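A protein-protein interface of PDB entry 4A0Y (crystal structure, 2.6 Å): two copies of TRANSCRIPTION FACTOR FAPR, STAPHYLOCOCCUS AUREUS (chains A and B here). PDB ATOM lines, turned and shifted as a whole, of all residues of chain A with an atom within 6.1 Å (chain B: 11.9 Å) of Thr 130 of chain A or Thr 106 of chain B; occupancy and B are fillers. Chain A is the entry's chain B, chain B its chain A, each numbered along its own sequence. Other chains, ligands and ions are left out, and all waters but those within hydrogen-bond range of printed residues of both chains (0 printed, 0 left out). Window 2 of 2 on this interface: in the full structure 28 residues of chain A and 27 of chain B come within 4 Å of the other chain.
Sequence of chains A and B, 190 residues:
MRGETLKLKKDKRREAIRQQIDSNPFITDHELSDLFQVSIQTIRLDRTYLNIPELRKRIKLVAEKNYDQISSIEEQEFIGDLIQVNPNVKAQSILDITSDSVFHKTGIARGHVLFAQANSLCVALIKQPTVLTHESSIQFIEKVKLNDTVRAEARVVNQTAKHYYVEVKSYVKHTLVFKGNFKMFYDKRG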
ATOM      1  N   GLN A 128     -17.464  34.265  27.833  1.00  0.00           N
ATOM      2  CA  GLN A 128     -18.468  34.357  26.776  1.00  0.00           C
ATOM      3  C   GLN A 128     -18.707  32.962  26.167  1.00  0.00           C
ATOM      4  O   GLN A 128     -17.782  32.139  26.121  1.00  0.00           O
ATOM      5  CB  GLN A 128     -18.056  35.382  25.698  1.00  0.00           C
ATOM      6  CG  GLN A 128     -17.840  36.784  26.200  1.00  0.00           C
ATOM      7  CD  GLN A 128     -19.111  37.474  26.653  1.00  0.00           C
ATOM      8  OE1 GLN A 128     -20.222  37.010  26.386  1.00  0.00           O
ATOM      9  NE2 GLN A 128     -18.954  38.603  27.328  1.00  0.00           N
ATOM     10  N   PRO A 129     -19.942  32.687  25.710  1.00  0.00           N
ATOM     11  CA  PRO A 129     -20.250  31.337  25.168  1.00  0.00           C
ATOM     12  C   PRO A 129     -19.297  30.901  24.042  1.00  0.00           C
ATOM     13  O   PRO A 129     -18.737  29.795  24.101  1.00  0.00           O
ATOM     14  CB  PRO A 129     -21.691  31.472  24.674  1.00  0.00           C
ATOM     15  CG  PRO A 129     -22.278  32.524  25.568  1.00  0.00           C
ATOM     16  CD  PRO A 129     -21.152  33.519  25.847  1.00  0.00           C
ATOM     17  N   THR A 130     -19.093  31.761  23.045  1.00  0.00           N
ATOM     18  CA  THR A 130     -18.014  31.526  22.098  1.00  0.00           C
ATOM     19  C   THR A 130     -17.046  32.720  21.948  1.00  0.00           C
ATOM     20  O   THR A 130     -17.450  33.901  21.910  1.00  0.00           O
ATOM     21  CB  THR A 130     -18.525  31.093  20.720  1.00  0.00           C
ATOM     22  OG1 THR A 130     -19.206  32.189  20.126  1.00  0.00           O
ATOM     23  CG2 THR A 130     -19.488  29.830  20.809  1.00  0.00           C
ATOM     24  N   VAL A 131     -15.769  32.350  21.832  1.00  0.00           N
ATOM     25  CA  VAL A 131     -14.643  33.226  21.767  1.00  0.00           C
ATOM     26  C   VAL A 131     -13.708  32.704  20.665  1.00  0.00           C
ATOM     27  O   VAL A 131     -13.120  31.609  20.797  1.00  0.00           O
ATOM     28  CB  VAL A 131     -13.905  33.236  23.141  1.00  0.00           C
ATOM     29  CG1 VAL A 131     -12.658  34.078  23.108  1.00  0.00           C
ATOM     30  CG2 VAL A 131     -14.834  33.746  24.222  1.00  0.00           C
ATOM     31  N   LEU A 132     -13.579  33.473  19.582  1.00  0.00           N
ATOM     32  CA  LEU A 132     -12.699  33.121  18.468  1.00  0.00           C
ATOM     33  C   LEU A 132     -11.606  34.167  18.292  1.00  0.00           C
ATOM     34  O   LEU A 132     -11.895  35.364  18.231  1.00  0.00           O
ATOM     35  CB  LEU A 132     -13.511  33.007  17.172  1.00  0.00           C
ATOM     36  CG  LEU A 132     -14.798  32.163  17.189  1.00  0.00           C
ATOM     37  CD1 LEU A 132     -15.493  32.149  15.821  1.00  0.00           C
ATOM     38  CD2 LEU A 132     -14.562  30.720  17.690  1.00  0.00           C
ATOM     39  N   PHE A 185     -12.771  37.779  19.003  1.00  0.00           N
ATOM     40  CA  PHE A 185     -14.204  37.887  18.725  1.00  0.00           C
ATOM     41  C   PHE A 185     -15.029  37.155  19.781  1.00  0.00           C
ATOM     42  O   PHE A 185     -14.613  36.135  20.303  1.00  0.00           O
ATOM     43  CB  PHE A 185     -14.499  37.349  17.339  1.00  0.00           C
ATOM     44  CG  PHE A 185     -15.944  37.290  17.029  1.00  0.00           C
ATOM     45  CD1 PHE A 185     -16.613  38.425  16.589  1.00  0.00           C
ATOM     46  CD2 PHE A 185     -16.668  36.073  17.187  1.00  0.00           C
ATOM     47  CE1 PHE A 185     -18.001  38.363  16.281  1.00  0.00           C
ATOM     48  CE2 PHE A 185     -18.022  36.005  16.909  1.00  0.00           C
ATOM     49  CZ  PHE A 185     -18.705  37.155  16.451  1.00  0.00           C
ATOM     50  N   TYR A 186     -16.186  37.680  20.137  1.00  0.00           N
ATOM     51  CA  TYR A 186     -17.058  36.882  20.978  1.00  0.00           C
ATOM     52  C   TYR A 186     -18.504  37.027  20.569  1.00  0.00           C
ATOM     53  O   TYR A 186     -18.848  37.911  19.794  1.00  0.00           O
ATOM     54  CB  TYR A 186     -16.865  37.201  22.452  1.00  0.00           C
ATOM     55  CG  TYR A 186     -17.432  38.524  22.862  1.00  0.00           C
ATOM     56  CD1 TYR A 186     -16.720  39.688  22.624  1.00  0.00           C
ATOM     57  CD2 TYR A 186     -18.680  38.621  23.487  1.00  0.00           C
ATOM     58  CE1 TYR A 186     -17.220  40.929  22.990  1.00  0.00           C
ATOM     59  CE2 TYR A 186     -19.194  39.862  23.879  1.00  0.00           C
ATOM     60  CZ  TYR A 186     -18.439  41.017  23.619  1.00  0.00           C
ATOM     61  OH  TYR A 186     -18.854  42.265  23.974  1.00  0.00           O
ATOM     62  N   ASP A 187     -19.335  36.134  21.100  1.00  0.00           N
ATOM     63  CA  ASP A 187     -20.785  36.131  20.879  1.00  0.00           C
ATOM     64  C   ASP A 187     -21.463  35.364  22.011  1.00  0.00           C
ATOM     65  O   ASP A 187     -20.898  34.377  22.515  1.00  0.00           O
ATOM     66  CB  ASP A 187     -21.075  35.392  19.579  1.00  0.00           C
ATOM     67  CG  ASP A 187     -22.362  35.841  18.920  1.00  0.00           C
ATOM     68  OD1 ASP A 187     -23.398  36.068  19.622  1.00  0.00           O
ATOM     69  OD2 ASP A 187     -22.344  35.935  17.667  1.00  0.00           O
ATOM     70  N   LYS A 188     -22.673  35.791  22.404  1.00  0.00           N
ATOM     71  CA  LYS A 188     -23.559  34.919  23.236  1.00  0.00           C
ATOM     72  C   LYS A 188     -24.473  34.017  22.414  1.00  0.00           C
ATOM     73  O   LYS A 188     -25.659  34.331  22.305  1.00  0.00           O
ATOM     74  CB  LYS A 188     -24.447  35.674  24.262  1.00  0.00           C
ATOM     75  CG  LYS A 188     -24.284  37.188  24.359  1.00  0.00           C
ATOM     76  CD  LYS A 188     -23.144  37.629  25.278  1.00  0.00           C
ATOM     77  CE  LYS A 188     -23.259  39.125  25.612  1.00  0.00           C
ATOM     78  NZ  LYS A 188     -23.598  39.924  24.389  1.00  0.00           N
ATOM     79  N   ARG A 189     -23.960  32.910  21.853  1.00  0.00           N
ATOM     80  CA  ARG A 189     -24.870  31.809  21.410  1.00  0.00           C
ATOM     81  C   ARG A 189     -25.128  30.728  22.491  1.00  0.00           C
ATOM     82  O   ARG A 189     -24.306  29.827  22.713  1.00  0.00           O
ATOM     83  CB  ARG A 189     -24.563  31.211  20.001  1.00  0.00           C
ATOM     84  CG  ARG A 189     -23.089  31.202  19.511  1.00  0.00           C
ATOM     85  CD  ARG A 189     -23.062  31.275  17.948  1.00  0.00           C
ATOM     86  NE  ARG A 189     -21.786  30.890  17.302  1.00  0.00           N
ATOM     87  CZ  ARG A 189     -20.873  31.726  16.771  1.00  0.00           C
ATOM     88  NH1 ARG A 189     -21.017  33.059  16.803  1.00  0.00           N
ATOM     89  NH2 ARG A 189     -19.782  31.215  16.206  1.00  0.00           N
ATOM     90  N   ILE B  97      -8.045  18.768  10.344  1.00  0.00           N
ATOM     91  CA  ILE B  97      -8.598  19.288  11.603  1.00  0.00           C
ATOM     92  C   ILE B  97      -9.484  18.254  12.337  1.00  0.00           C
ATOM     93  O   ILE B  97     -10.603  17.955  11.931  1.00  0.00           O
ATOM     94  CB  ILE B  97      -9.416  20.550  11.302  1.00  0.00           C
ATOM     95  CG1 ILE B  97      -8.535  21.590  10.616  1.00  0.00           C
ATOM     96  CG2 ILE B  97     -10.089  21.097  12.536  1.00  0.00           C
ATOM     97  CD1 ILE B  97      -7.467  22.258  11.518  1.00  0.00           C
ATOM     98  N   THR B  98      -9.007  17.710  13.432  1.00  0.00           N
ATOM     99  CA  THR B  98      -9.786  16.720  14.124  1.00  0.00           C
ATOM    100  C   THR B  98     -10.460  17.266  15.407  1.00  0.00           C
ATOM    101  O   THR B  98     -10.194  18.411  15.850  1.00  0.00           O
ATOM    102  CB  THR B  98      -8.903  15.510  14.504  1.00  0.00           C
ATOM    103  OG1 THR B  98      -8.138  15.843  15.668  1.00  0.00           O
ATOM    104  CG2 THR B  98      -7.976  15.080  13.376  1.00  0.00           C
ATOM    105  N   SER B  99     -11.297  16.437  16.017  1.00  0.00           N
ATOM    106  CA  SER B  99     -12.086  16.799  17.165  1.00  0.00           C
ATOM    107  C   SER B  99     -11.285  17.469  18.307  1.00  0.00           C
ATOM    108  O   SER B  99     -11.798  18.332  19.001  1.00  0.00           O
ATOM    109  CB  SER B  99     -12.813  15.568  17.650  1.00  0.00           C
ATOM    110  OG  SER B  99     -12.797  15.479  19.042  1.00  0.00           O
ATOM    111  N   ASP B 100     -10.019  17.110  18.477  1.00  0.00           N
ATOM    112  CA  ASP B 100      -9.232  17.673  19.557  1.00  0.00           C
ATOM    113  C   ASP B 100      -8.800  19.089  19.250  1.00  0.00           C
ATOM    114  O   ASP B 100      -8.313  19.774  20.123  1.00  0.00           O
ATOM    115  CB  ASP B 100      -7.985  16.850  19.828  1.00  0.00           C
ATOM    116  CG  ASP B 100      -8.277  15.536  20.501  1.00  0.00           C
ATOM    117  OD1 ASP B 100      -9.391  15.295  21.078  1.00  0.00           O
ATOM    118  OD2 ASP B 100      -7.347  14.709  20.441  1.00  0.00           O
ATOM    119  N   SER B 101      -8.943  19.542  18.017  1.00  0.00           N
ATOM    120  CA  SER B 101      -8.539  20.871  17.708  1.00  0.00           C
ATOM    121  C   SER B 101      -9.687  21.833  17.701  1.00  0.00           C
ATOM    122  O   SER B 101      -9.487  22.993  17.326  1.00  0.00           O
ATOM    123  CB  SER B 101      -7.900  20.894  16.349  1.00  0.00           C
ATOM    124  OG  SER B 101      -6.767  20.082  16.388  1.00  0.00           O
ATOM    125  N   VAL B 102     -10.885  21.397  18.078  1.00  0.00           N
ATOM    126  CA  VAL B 102     -12.033  22.262  17.926  1.00  0.00           C
ATOM    127  C   VAL B 102     -12.886  22.351  19.178  1.00  0.00           C
ATOM    128  O   VAL B 102     -12.891  21.417  20.005  1.00  0.00           O
ATOM    129  CB  VAL B 102     -12.951  21.811  16.738  1.00  0.00           C
ATOM    130  CG1 VAL B 102     -12.170  21.709  15.435  1.00  0.00           C
ATOM    131  CG2 VAL B 102     -13.738  20.516  17.078  1.00  0.00           C
ATOM    132  N   PHE B 103     -13.657  23.442  19.283  1.00  0.00           N
ATOM    133  CA  PHE B 103     -14.657  23.584  20.352  1.00  0.00           C
ATOM    134  C   PHE B 103     -15.795  22.606  20.156  1.00  0.00           C
ATOM    135  O   PHE B 103     -16.187  22.342  19.029  1.00  0.00           O
ATOM    136  CB  PHE B 103     -15.193  25.018  20.433  1.00  0.00           C
ATOM    137  CG  PHE B 103     -14.092  26.099  20.589  1.00  0.00           C
ATOM    138  CD1 PHE B 103     -13.553  26.399  21.844  1.00  0.00           C
ATOM    139  CD2 PHE B 103     -13.659  26.828  19.490  1.00  0.00           C
ATOM    140  CE1 PHE B 103     -12.571  27.357  22.001  1.00  0.00           C
ATOM    141  CE2 PHE B 103     -12.669  27.825  19.614  1.00  0.00           C
ATOM    142  CZ  PHE B 103     -12.110  28.103  20.882  1.00  0.00           C
ATOM    143  N   HIS B 104     -16.327  22.081  21.258  1.00  0.00           N
ATOM    144  CA  HIS B 104     -17.347  21.072  21.240  1.00  0.00           C
ATOM    145  C   HIS B 104     -18.641  21.527  20.575  1.00  0.00           C
ATOM    146  O   HIS B 104     -19.249  20.767  19.791  1.00  0.00           O
ATOM    147  CB  HIS B 104     -17.611  20.568  22.667  1.00  0.00           C
ATOM    148  CG  HIS B 104     -18.765  19.602  22.780  1.00  0.00           C
ATOM    149  ND1 HIS B 104     -18.842  18.427  22.051  1.00  0.00           N
ATOM    150  CD2 HIS B 104     -19.869  19.621  23.564  1.00  0.00           C
ATOM    151  CE1 HIS B 104     -19.944  17.768  22.376  1.00  0.00           C
ATOM    152  NE2 HIS B 104     -20.583  18.466  23.297  1.00  0.00           N
ATOM    153  N   LYS B 105     -19.100  22.736  20.925  1.00  0.00           N
ATOM    154  CA  LYS B 105     -20.446  23.210  20.490  1.00  0.00           C
ATOM    155  C   LYS B 105     -20.428  23.551  19.003  1.00  0.00           C
ATOM    156  O   LYS B 105     -21.344  23.197  18.293  1.00  0.00           O
ATOM    157  CB  LYS B 105     -20.952  24.449  21.284  1.00  0.00           C
ATOM    158  CG  LYS B 105     -21.202  24.310  22.802  1.00  0.00           C
ATOM    159  CD  LYS B 105     -22.306  23.220  23.135  1.00  0.00           C
ATOM    160  CE  LYS B 105     -23.253  23.625  24.319  1.00  0.00           C
ATOM    161  NZ  LYS B 105     -22.638  24.812  25.095  1.00  0.00           N
ATOM    162  N   THR B 106     -19.380  24.232  18.542  1.00  0.00           N
ATOM    163  CA  THR B 106     -19.394  24.784  17.200  1.00  0.00           C
ATOM    164  C   THR B 106     -18.574  24.031  16.169  1.00  0.00           C
ATOM    165  O   THR B 106     -18.909  24.049  14.991  1.00  0.00           O
ATOM    166  CB  THR B 106     -18.924  26.211  17.202  1.00  0.00           C
ATOM    167  OG1 THR B 106     -17.575  26.243  17.657  1.00  0.00           O
ATOM    168  CG2 THR B 106     -19.790  27.021  18.116  1.00  0.00           C
ATOM    169  N   GLY B 107     -17.503  23.387  16.599  1.00  0.00           N
ATOM    170  CA  GLY B 107     -16.699  22.622  15.704  1.00  0.00           C
ATOM    171  C   GLY B 107     -15.661  23.494  15.071  1.00  0.00           C
ATOM    172  O   GLY B 107     -15.056  23.115  14.067  1.00  0.00           O
ATOM    173  N   ILE B 108     -15.440  24.669  15.647  1.00  0.00           N
ATOM    174  CA  ILE B 108     -14.498  25.606  15.063  1.00  0.00           C
ATOM    175  C   ILE B 108     -13.087  25.324  15.607  1.00  0.00           C
ATOM    176  O   ILE B 108     -12.921  25.082  16.798  1.00  0.00           O
ATOM    177  CB  ILE B 108     -14.936  27.084  15.298  1.00  0.00           C
ATOM    178  CG1 ILE B 108     -16.245  27.370  14.574  1.00  0.00           C
ATOM    179  CG2 ILE B 108     -13.871  28.059  14.791  1.00  0.00           C
ATOM    180  CD1 ILE B 108     -16.987  28.536  15.170  1.00  0.00           C
ATOM    181  N   ALA B 109     -12.087  25.344  14.730  1.00  0.00           N
ATOM    182  CA  ALA B 109     -10.711  25.136  15.137  1.00  0.00           C
ATOM    183  C   ALA B 109     -10.251  26.217  16.102  1.00  0.00           C
ATOM    184  O   ALA B 109     -10.537  27.393  15.889  1.00  0.00           O
ATOM    185  CB  ALA B 109      -9.829  25.115  13.928  1.00  0.00           C
ATOM    186  N   ARG B 110      -9.561  25.830  17.178  1.00  0.00           N
ATOM    187  CA  ARG B 110      -8.952  26.794  18.091  1.00  0.00           C
ATOM    188  C   ARG B 110      -7.868  27.619  17.416  1.00  0.00           C
ATOM    189  O   ARG B 110      -7.174  27.148  16.509  1.00  0.00           O
ATOM    190  CB  ARG B 110      -8.398  26.076  19.306  1.00  0.00           C
ATOM    191  CG  ARG B 110      -9.509  25.443  20.084  1.00  0.00           C
ATOM    192  CD  ARG B 110      -9.057  24.514  21.187  1.00  0.00           C
ATOM    193  NE  ARG B 110     -10.096  24.498  22.207  1.00  0.00           N
ATOM    194  CZ  ARG B 110     -10.855  23.453  22.501  1.00  0.00           C
ATOM    195  NH1 ARG B 110     -10.670  22.279  21.891  1.00  0.00           N
ATOM    196  NH2 ARG B 110     -11.794  23.581  23.434  1.00  0.00           N
ATOM    197  N   GLY B 111      -7.694  28.854  17.882  1.00  0.00           N
ATOM    198  CA  GLY B 111      -6.683  29.761  17.285  1.00  0.00           C
ATOM    199  C   GLY B 111      -5.248  29.226  17.173  1.00  0.00           C
ATOM    200  O   GLY B 111      -4.534  29.410  16.123  1.00  0.00           O
ATOM    201  N   GLU B 142     -11.343  33.213   8.039  1.00  0.00           N
ATOM    202  CA  GLU B 142     -12.647  32.504   8.062  1.00  0.00           C
ATOM    203  C   GLU B 142     -12.593  31.432   9.131  1.00  0.00           C
ATOM    204  O   GLU B 142     -11.522  30.928   9.412  1.00  0.00           O
ATOM    205  CB  GLU B 142     -12.932  31.789   6.744  1.00  0.00           C
ATOM    206  CG  GLU B 142     -12.713  32.598   5.457  1.00  0.00           C
ATOM    207  CD  GLU B 142     -13.810  33.642   5.171  1.00  0.00           C
ATOM    208  OE1 GLU B 142     -14.817  33.670   5.922  1.00  0.00           O
ATOM    209  OE2 GLU B 142     -13.654  34.437   4.199  1.00  0.00           O
ATOM    210  N   LYS B 143     -13.738  31.067   9.716  1.00  0.00           N
ATOM    211  CA  LYS B 143     -13.808  29.927  10.632  1.00  0.00           C
ATOM    212  C   LYS B 143     -13.318  28.622   9.950  1.00  0.00           C
ATOM    213  O   LYS B 143     -13.802  28.268   8.880  1.00  0.00           O
ATOM    214  CB  LYS B 143     -15.238  29.707  11.084  1.00  0.00           C
ATOM    215  CG  LYS B 143     -15.946  30.866  11.791  1.00  0.00           C
ATOM    216  CD  LYS B 143     -17.445  30.423  11.925  1.00  0.00           C
ATOM    217  CE  LYS B 143     -18.507  31.558  11.881  1.00  0.00           C
ATOM    218  NZ  LYS B 143     -18.510  32.325  13.165  1.00  0.00           N
ATOM    219  N   VAL B 144     -12.352  27.932  10.547  1.00  0.00           N
ATOM    220  CA  VAL B 144     -12.001  26.573  10.122  1.00  0.00           C
ATOM    221  C   VAL B 144     -12.798  25.532  10.917  1.00  0.00           C
ATOM    222  O   VAL B 144     -13.005  25.672  12.128  1.00  0.00           O
ATOM    223  CB  VAL B 144     -10.492  26.339  10.294  1.00  0.00           C
ATOM    224  CG1 VAL B 144     -10.125  24.878  10.130  1.00  0.00           C
ATOM    225  CG2 VAL B 144      -9.718  27.203   9.294  1.00  0.00           C
ATOM    226  N   LYS B 145     -13.238  24.479  10.254  1.00  0.00           N
ATOM    227  CA  LYS B 145     -14.168  23.546  10.881  1.00  0.00           C
ATOM    228  C   LYS B 145     -13.668  22.109  11.036  1.00  0.00           C
ATOM    229  O   LYS B 145     -12.800  21.637  10.280  1.00  0.00           O
ATOM    230  CB  LYS B 145     -15.494  23.543  10.105  1.00  0.00           C
ATOM    231  CG  LYS B 145     -16.198  24.881  10.101  1.00  0.00           C
ATOM    232  CD  LYS B 145     -17.057  24.980  11.337  1.00  0.00           C
ATOM    233  CE  LYS B 145     -18.411  25.643  11.033  1.00  0.00           C
ATOM    234  NZ  LYS B 145     -19.499  24.785  11.628  1.00  0.00           N
ATOM    235  N   LEU B 146     -14.267  21.403  11.989  1.00  0.00           N
ATOM    236  CA  LEU B 146     -14.019  19.990  12.163  1.00  0.00           C
ATOM    237  C   LEU B 146     -14.014  19.253  10.836  1.00  0.00           C
ATOM    238  O   LEU B 146     -14.982  19.364  10.072  1.00  0.00           O
ATOM    239  CB  LEU B 146     -15.102  19.383  13.043  1.00  0.00           C
ATOM    240  CG  LEU B 146     -15.104  17.856  13.192  1.00  0.00           C
ATOM    241  CD1 LEU B 146     -13.778  17.357  13.790  1.00  0.00           C
ATOM    242  CD2 LEU B 146     -16.272  17.415  14.045  1.00  0.00           C
ATOM    243  N   ASN B 147     -12.952  18.483  10.585  1.00  0.00           N
ATOM    244  CA  ASN B 147     -12.787  17.635   9.372  1.00  0.00           C
ATOM    245  C   ASN B 147     -12.442  18.378   8.083  1.00  0.00           C
ATOM    246  O   ASN B 147     -12.407  17.787   7.032  1.00  0.00           O
ATOM    247  CB  ASN B 147     -13.953  16.676   9.110  1.00  0.00           C
ATOM    248  CG  ASN B 147     -14.080  15.540  10.165  1.00  0.00           C
ATOM    249  OD1 ASN B 147     -13.085  14.988  10.673  1.00  0.00           O
ATOM    250  ND2 ASN B 147     -15.332  15.172  10.466  1.00  0.00           N
ATOM    251  N   ASP B 148     -12.170  19.669   8.173  1.00  0.00           N
ATOM    252  CA  ASP B 148     -11.535  20.415   7.092  1.00  0.00           C
ATOM    253  C   ASP B 148     -10.063  20.013   6.980  1.00  0.00           C
ATOM    254  O   ASP B 148      -9.474  19.536   7.956  1.00  0.00           O
ATOM    255  CB  ASP B 148     -11.570  21.914   7.410  1.00  0.00           C
ATOM    256  CG  ASP B 148     -12.905  22.581   7.066  1.00  0.00           C
ATOM    257  OD1 ASP B 148     -13.820  22.007   6.328  1.00  0.00           O
ATOM    258  OD2 ASP B 148     -12.996  23.733   7.539  1.00  0.00           O
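The guanidinium group (NH2) of Arg 189 of chain A lies close to the side-chain amino group (NZ) of Lys 143 of chain B, 3.5 Å away.
The backbone NH of Phe 103 of chain B lies within hydrogen-bond range of the backbone carbonyl oxygen of Ile 108 of chain B (3.1 Å). The backbone NH of Ile 108 of chain B lies close to the side-chain hydroxyl of Thr 106 of chain B. The side-chain amino group (NZ) of Lys 145 of chain B sits at hydrogen-bond distance from the backbone carbonyl oxygen (O) of Thr 106 of chain B, at 3.5 Å. O of Thr 130 of chain A lies within hydrogen-bond range of N of Asp 187 of chain A (3.0 Å). N of Phe 185 of chain A sits at hydrogen-bond distance from O of Leu 132 of chain A (2.7 Å). The side-chain carboxylate (OD2) of Asp 187 of chain A is in salt-bridge range of the guanidinium group (NH1) of Arg 189 of chain A (3.3 Å).
Among the printed residues, pairs that only touch across the chains: Val 131 of chain A with Phe 103 of chain B, Thr 130 of chain A with Thr 106 of chain B, Leu 132 of chain A with Phe 103 of chain B and Leu 132 of chain A with Ile 108 of chain B.
Thr 130 of chain A touches just one residue of chain B: Thr 106 (3.9 Å). Of chain A, only Thr 130 (3.9 Å) comes within 4 Å of Thr 106 of chain B. No residue of chain B comes within 4 Å of Gln 128 of chain A. No residue of chain B comes within 4 Å of Pro 129 of chain A. Val 131 of chain A touches just one residue of chain B: Phe 103. Leu 132 of chain A touches two residues of chain B. No residue of chain B comes within 4 Å of Phe 185 of chain A. No residue of chain B comes within 4 Å of Asp 187 of chain A. Printed residues of chain B within 4 Å of Arg 189 of chain A: Lys 143. Of the printed residues of chain A, Lys 143 of chain B touches Arg 189 (3.5 Å). Glu 142 of chain B touches none of the printed residues of chain A. The nearest residue of chain A that does not touch Thr 106 of chain B is Arg 189 of chain A (4.4 Å). The nearest printed residue of chain B that does not touch Arg 189 of chain A is Ile 108 of chain B (4.01 Å).
Printed residues of chain B that touch a printed residue of chain A: Phe 103, Thr 106, Ile 108 and Lys 143. Of the 10 printed residues of chain A, 4 touch a printed residue of chain B. Printed residues of chain A that touch a printed residue of chain B: Thr 130, Val 131, Leu 132 and Arg 189. Hydrophobic or aromatic side chains of chain A within 4 Å of the printed part of chain B: Leu 132. Along chain A the printed residues that touch a printed residue of chain B span positions 130 to 189. Among the printed residues, 5 pairs touch across the chains. Among the printed residues, no Asp or Glu carboxylate lies within 4 Å of a Lys or Arg side-chain nitrogen of the other chain.
No position is printed for both chains.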
